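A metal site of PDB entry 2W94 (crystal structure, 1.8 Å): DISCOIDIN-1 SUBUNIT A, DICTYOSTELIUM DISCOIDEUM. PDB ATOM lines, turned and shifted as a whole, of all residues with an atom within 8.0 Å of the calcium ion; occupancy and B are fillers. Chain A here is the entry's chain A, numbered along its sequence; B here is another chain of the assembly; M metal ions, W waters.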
ATOM      1  N   GLY A 163     -13.004 -17.846  12.661  1.00  0.00           N
ATOM      2  CA  GLY A 163     -11.904 -16.941  12.917  1.00  0.00           C
ATOM      3  C   GLY A 163     -11.465 -16.302  11.605  1.00  0.00           C
ATOM      4  O   GLY A 163     -11.331 -16.976  10.596  1.00  0.00           O
ATOM      5  N   ALA A 164     -11.236 -14.995  11.640  1.00  0.00           N
ATOM      6  CA  ALA A 164     -10.982 -14.255  10.440  1.00  0.00           C
ATOM      7  C   ALA A 164      -9.530 -13.791  10.315  1.00  0.00           C
ATOM      8  O   ALA A 164      -8.854 -13.524  11.332  1.00  0.00           O
ATOM      9  CB  ALA A 164     -11.889 -13.069  10.359  1.00  0.00           C
ATOM     10  N   ASP A 165      -9.074 -13.812   9.063  1.00  0.00           N
ATOM     11  CA  ASP A 165      -7.884 -13.069   8.635  1.00  0.00           C
ATOM     12  C   ASP A 165      -6.529 -13.554   9.176  1.00  0.00           C
ATOM     13  O   ASP A 165      -5.675 -12.742   9.604  1.00  0.00           O
ATOM     14  CB  ASP A 165      -8.064 -11.592   8.885  1.00  0.00           C
ATOM     15  CG  ASP A 165      -9.376 -11.060   8.350  1.00  0.00           C
ATOM     16  OD1 ASP A 165      -9.944 -11.590   7.382  1.00  0.00           O
ATOM     17  OD2 ASP A 165      -9.830 -10.070   8.938  1.00  0.00           O
ATOM     18  N   ILE A 166      -6.318 -14.855   9.097  1.00  0.00           N
ATOM     19  CA  ILE A 166      -5.040 -15.450   9.419  1.00  0.00           C
ATOM     20  C   ILE A 166      -4.105 -15.088   8.259  1.00  0.00           C
ATOM     21  O   ILE A 166      -4.451 -15.377   7.118  1.00  0.00           O
ATOM     22  CB  ILE A 166      -5.141 -16.970   9.551  1.00  0.00           C
ATOM     23  CG1 ILE A 166      -6.351 -17.377  10.426  1.00  0.00           C
ATOM     24  CG2 ILE A 166      -3.833 -17.511  10.109  1.00  0.00           C
ATOM     25  CD1 ILE A 166      -6.514 -16.537  11.722  1.00  0.00           C
ATOM     26  N   ASN A 202      -9.690 -21.367   4.172  1.00  0.00           N
ATOM     27  CA  ASN A 202      -9.904 -20.983   2.768  1.00  0.00           C
ATOM     28  C   ASN A 202      -9.441 -19.585   2.484  1.00  0.00           C
ATOM     29  O   ASN A 202      -9.430 -18.756   3.352  1.00  0.00           O
ATOM     30  CB  ASN A 202     -11.391 -21.108   2.399  1.00  0.00           C
ATOM     31  CG  ASN A 202     -11.897 -22.535   2.521  1.00  0.00           C
ATOM     32  OD1 ASN A 202     -12.891 -22.786   3.208  1.00  0.00           O
ATOM     33  ND2 ASN A 202     -11.224 -23.472   1.865  1.00  0.00           N
ATOM     34  N   PHE A 203      -9.068 -19.283   1.235  1.00  0.00           N
ATOM     35  CA  PHE A 203      -8.403 -18.013   0.962  1.00  0.00           C
ATOM     36  C   PHE A 203      -9.376 -16.836   0.931  1.00  0.00           C
ATOM     37  O   PHE A 203     -10.481 -16.957   0.442  1.00  0.00           O
ATOM     38  CB  PHE A 203      -7.755 -18.048  -0.430  1.00  0.00           C
ATOM     39  CG  PHE A 203      -6.669 -19.049  -0.606  1.00  0.00           C
ATOM     40  CD1 PHE A 203      -6.823 -20.098  -1.510  1.00  0.00           C
ATOM     41  CD2 PHE A 203      -5.468 -18.887   0.044  1.00  0.00           C
ATOM     42  CE1 PHE A 203      -5.829 -21.001  -1.690  1.00  0.00           C
ATOM     43  CE2 PHE A 203      -4.450 -19.772  -0.179  1.00  0.00           C
ATOM     44  CZ  PHE A 203      -4.624 -20.844  -1.024  1.00  0.00           C
ATOM     45  N   ASP A 204      -8.947 -15.674   1.402  1.00  0.00           N
ATOM     46  CA  ASP A 204      -9.665 -14.449   1.157  1.00  0.00           C
ATOM     47  C   ASP A 204      -8.785 -13.332   0.568  1.00  0.00           C
ATOM     48  O   ASP A 204      -9.310 -12.321   0.153  1.00  0.00           O
ATOM     49  CB  ASP A 204     -10.350 -13.925   2.436  1.00  0.00           C
ATOM     50  CG  ASP A 204      -9.396 -13.462   3.465  1.00  0.00           C
ATOM     51  OD1 ASP A 204      -8.250 -13.927   3.474  1.00  0.00           O
ATOM     52  OD2 ASP A 204      -9.780 -12.600   4.305  1.00  0.00           O
ATOM     53  N   GLN A 205      -7.451 -13.506   0.572  1.00  0.00           N
ATOM     54  CA  GLN A 205      -6.569 -12.484  -0.086  1.00  0.00           C
ATOM     55  C   GLN A 205      -5.364 -13.212  -0.677  1.00  0.00           C
ATOM     56  O   GLN A 205      -4.649 -13.914   0.044  1.00  0.00           O
ATOM     57  CB  GLN A 205      -6.116 -11.399   0.882  1.00  0.00           C
ATOM     58  CG  GLN A 205      -5.553 -10.163   0.192  1.00  0.00           C
ATOM     59  CD  GLN A 205      -5.075  -9.088   1.152  1.00  0.00           C
ATOM     60  OE1 GLN A 205      -5.775  -8.123   1.450  1.00  0.00           O
ATOM     61  NE2 GLN A 205      -3.881  -9.278   1.710  1.00  0.00           N
ATOM     62  N   ARG A 245      -3.877 -14.732   2.729  1.00  0.00           N
ATOM     63  CA  ARG A 245      -4.683 -14.631   3.917  1.00  0.00           C
ATOM     64  C   ARG A 245      -5.818 -15.611   3.799  1.00  0.00           C
ATOM     65  O   ARG A 245      -6.271 -15.937   2.712  1.00  0.00           O
ATOM     66  CB  ARG A 245      -5.215 -13.224   4.077  1.00  0.00           C
ATOM     67  CG  ARG A 245      -5.646 -12.843   5.489  1.00  0.00           C
ATOM     68  CD  ARG A 245      -6.147 -11.342   5.500  1.00  0.00           C
ATOM     69  NE  ARG A 245      -7.335 -11.197   4.689  1.00  0.00           N
ATOM     70  CZ  ARG A 245      -7.719 -10.082   4.104  1.00  0.00           C
ATOM     71  NH1 ARG A 245      -6.990  -8.986   4.207  1.00  0.00           N
ATOM     72  NH2 ARG A 245      -8.808 -10.073   3.362  1.00  0.00           N
ATOM     73  N   ALA A 246      -6.328 -16.032   4.944  1.00  0.00           N
ATOM     74  CA  ALA A 246      -7.390 -17.011   4.991  1.00  0.00           C
ATOM     75  C   ALA A 246      -8.261 -16.791   6.227  1.00  0.00           C
ATOM     76  O   ALA A 246      -7.828 -16.245   7.199  1.00  0.00           O
ATOM     77  CB  ALA A 246      -6.801 -18.456   5.035  1.00  0.00           C
ATOM     78  N   ASP A 247      -9.505 -17.251   6.145  1.00  0.00           N
ATOM     79  CA  ASP A 247     -10.419 -17.289   7.310  1.00  0.00           C
ATOM     80  C   ASP A 247     -10.693 -18.772   7.568  1.00  0.00           C
ATOM     81  O   ASP A 247     -10.603 -19.580   6.648  1.00  0.00           O
ATOM     82  CB  ASP A 247     -11.756 -16.671   6.952  1.00  0.00           C
ATOM     83  CG  ASP A 247     -11.677 -15.195   6.598  1.00  0.00           C
ATOM     84  OD1 ASP A 247     -10.833 -14.481   7.108  1.00  0.00           O
ATOM     85  OD2 ASP A 247     -12.495 -14.788   5.788  1.00  0.00           O
ATOM     86  N   TYR A 248     -11.055 -19.135   8.801  1.00  0.00           N
ATOM     87  CA  TYR A 248     -11.363 -20.506   9.135  1.00  0.00           C
ATOM     88  C   TYR A 248     -12.742 -20.665   9.757  1.00  0.00           C
ATOM     89  O   TYR A 248     -13.290 -19.752  10.365  1.00  0.00           O
ATOM     90  CB  TYR A 248     -10.322 -21.132  10.071  1.00  0.00           C
ATOM     91  CG  TYR A 248     -10.330 -20.632  11.516  1.00  0.00           C
ATOM     92  CD1 TYR A 248      -9.512 -19.597  11.922  1.00  0.00           C
ATOM     93  CD2 TYR A 248     -11.140 -21.245  12.464  1.00  0.00           C
ATOM     94  CE1 TYR A 248      -9.481 -19.190  13.215  1.00  0.00           C
ATOM     95  CE2 TYR A 248     -11.124 -20.841  13.742  1.00  0.00           C
ATOM     96  CZ  TYR A 248     -10.298 -19.816  14.135  1.00  0.00           C
ATOM     97  OH  TYR A 248     -10.305 -19.430  15.456  1.00  0.00           O
ATOM     98  N   VAL B 199     -17.431 -13.366  10.747  1.00  0.00           N
ATOM     99  CA  VAL B 199     -17.747 -13.730   9.362  1.00  0.00           C
ATOM    100  C   VAL B 199     -16.499 -14.168   8.604  1.00  0.00           C
ATOM    101  O   VAL B 199     -15.537 -13.383   8.502  1.00  0.00           O
ATOM    102  CB  VAL B 199     -18.430 -12.564   8.572  1.00  0.00           C
ATOM    103  CG1 VAL B 199     -18.738 -12.973   7.146  1.00  0.00           C
ATOM    104  CG2 VAL B 199     -19.720 -12.088   9.214  1.00  0.00           C
ATOM    105  N   ALA B 200     -16.535 -15.405   8.109  1.00  0.00           N
ATOM    106  CA  ALA B 200     -15.621 -15.939   7.088  1.00  0.00           C
ATOM    107  C   ALA B 200     -16.214 -15.641   5.694  1.00  0.00           C
ATOM    108  O   ALA B 200     -17.403 -15.862   5.464  1.00  0.00           O
ATOM    109  CB  ALA B 200     -15.431 -17.448   7.267  1.00  0.00           C
ATOM    110  N   LEU B 201     -15.381 -15.142   4.778  1.00  0.00           N
ATOM    111  CA  LEU B 201     -15.819 -14.817   3.434  1.00  0.00           C
ATOM    112  C   LEU B 201     -14.657 -15.120   2.486  1.00  0.00           C
ATOM    113  O   LEU B 201     -13.561 -14.521   2.584  1.00  0.00           O
ATOM    114  CB  LEU B 201     -16.228 -13.341   3.392  1.00  0.00           C
ATOM    115  CG  LEU B 201     -16.660 -12.674   2.106  1.00  0.00           C
ATOM    116  CD1 LEU B 201     -17.986 -13.124   1.617  1.00  0.00           C
ATOM    117  CD2 LEU B 201     -16.643 -11.155   2.396  1.00  0.00           C
ATOM    118  N   ASN B 202     -14.879 -16.141   1.675  1.00  0.00           N
ATOM    119  CA  ASN B 202     -13.812 -16.784   0.895  1.00  0.00           C
ATOM    120  C   ASN B 202     -14.223 -17.032  -0.548  1.00  0.00           C
ATOM    121  O   ASN B 202     -15.416 -17.126  -0.860  1.00  0.00           O
ATOM    122  CB  ASN B 202     -13.388 -18.073   1.575  1.00  0.00           C
ATOM    123  CG  ASN B 202     -13.053 -17.890   3.031  1.00  0.00           C
ATOM    124  OD1 ASN B 202     -13.702 -18.501   3.889  1.00  0.00           O
ATOM    125  ND2 ASN B 202     -12.075 -17.050   3.330  1.00  0.00           N
ATOM    126  N   VAL B 219     -11.155 -10.308  -0.788  1.00  0.00           N
ATOM    127  CA  VAL B 219     -12.550 -10.107  -0.377  1.00  0.00           C
ATOM    128  C   VAL B 219     -12.531 -10.059   1.160  1.00  0.00           C
ATOM    129  O   VAL B 219     -11.784 -10.788   1.796  1.00  0.00           O
ATOM    130  CB  VAL B 219     -13.479 -11.201  -0.921  1.00  0.00           C
ATOM    131  CG1 VAL B 219     -13.140 -12.572  -0.349  1.00  0.00           C
ATOM    132  CG2 VAL B 219     -14.926 -10.853  -0.661  1.00  0.00           C
ATOM    133  N   GLN B 220     -13.347  -9.164   1.727  1.00  0.00           N
ATOM    134  CA  GLN B 220     -13.401  -8.934   3.154  1.00  0.00           C
ATOM    135  C   GLN B 220     -14.758  -8.311   3.555  1.00  0.00           C
ATOM    136  O   GLN B 220     -15.295  -7.436   2.841  1.00  0.00           O
ATOM    137  CB  GLN B 220     -12.216  -7.995   3.527  1.00  0.00           C
ATOM    138  CG  GLN B 220     -12.014  -7.741   5.000  1.00  0.00           C
ATOM    139  CD  GLN B 220     -11.502  -8.952   5.762  1.00  0.00           C
ATOM    140  OE1 GLN B 220     -11.588 -10.075   5.296  1.00  0.00           O
ATOM    141  NE2 GLN B 220     -10.970  -8.712   6.964  1.00  0.00           N
ATOM    142  N   PRO B 221     -15.300  -8.726   4.717  1.00  0.00           N
ATOM    143  CA  PRO B 221     -16.489  -8.063   5.263  1.00  0.00           C
ATOM    144  C   PRO B 221     -16.135  -6.713   5.863  1.00  0.00           C
ATOM    145  O   PRO B 221     -15.041  -6.532   6.412  1.00  0.00           O
ATOM    146  CB  PRO B 221     -16.960  -9.038   6.344  1.00  0.00           C
ATOM    147  CG  PRO B 221     -16.177 -10.319   6.152  1.00  0.00           C
ATOM    148  CD  PRO B 221     -14.886  -9.866   5.530  1.00  0.00           C
ATOM    149  N   TYR B 234     -11.966  -6.550  -3.818  1.00  0.00           N
ATOM    150  CA  TYR B 234     -10.942  -5.577  -4.176  1.00  0.00           C
ATOM    151  C   TYR B 234      -9.720  -6.134  -4.924  1.00  0.00           C
ATOM    152  O   TYR B 234      -9.428  -7.333  -4.950  1.00  0.00           O
ATOM    153  CB  TYR B 234     -10.511  -4.769  -2.966  1.00  0.00           C
ATOM    154  CG  TYR B 234      -9.948  -5.592  -1.842  1.00  0.00           C
ATOM    155  CD1 TYR B 234      -8.592  -5.822  -1.737  1.00  0.00           C
ATOM    156  CD2 TYR B 234     -10.791  -6.220  -0.904  1.00  0.00           C
ATOM    157  CE1 TYR B 234      -8.061  -6.610  -0.719  1.00  0.00           C
ATOM    158  CE2 TYR B 234     -10.267  -6.997   0.126  1.00  0.00           C
ATOM    159  CZ  TYR B 234      -8.908  -7.220   0.207  1.00  0.00           C
ATOM    160  OH  TYR B 234      -8.367  -7.986   1.231  1.00  0.00           O
HETATM  161 CA    CA M   1     -11.532 -12.403   5.938  1.00  0.00          CA
HETATM  162  O   HOH W   1     -13.218 -12.035   7.552  1.00  0.00           O
HETATM  163  O   HOH W   2     -12.862 -12.310   3.928  1.00  0.00           O
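Water W2 bridges O of Leu 201 of chain B (2.7 Å) and O of Val 219 of chain B (2.8 Å).
The side-chain amide oxygen of Gln 220 of chain B lies close to the guanidinium group of Arg 245, 3.4 Å away. The guanidinium group of Arg 245 sits close to the side-chain carboxylate of Asp 165 (3.8 Å). The side-chain carboxylate of Asp 247 lies close to the backbone NH of Leu 201 of chain B, 3.1 Å away. OD1 of Asp 204 is in hydrogen-bond range of N of Ala 246, 3.2 Å away. N of Val 219 of chain B is in hydrogen-bond range of O of Asp 204 (2.9 Å). The side-chain amide nitrogen (ND2) of Asn 202 of chain B lies close to the side-chain carboxylate (OD2) of Asp 247 (3.4 Å). The backbone NH (N) of Asp 247 sits at hydrogen-bond distance from the backbone carbonyl oxygen (O) of Asn 202 of chain A, 3.2 Å away. OD1 of Asp 204 lies within salt-bridge range of NE of Arg 245 (3.1 Å).
The calcium ion is bound by OD1 of Asp 165 (2.3 Å), water W1 (2.4 Å), OD2 of Asp 204 (2.4 Å), water W2 (2.4 Å), OE1 of Gln 220 of chain B (2.4 Å), OD1 of Asp 247 (2.5 Å) and OD2 of Asp 247 (2.6 Å).
Four residues have an atom within 4 Å of the calcium ion: Asp 165, Asp 204, Asp 247 and Gln 220 of chain B. The nearest printed residue that does not touch the calcium ion is Pro 221 of chain B (4.2 Å).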
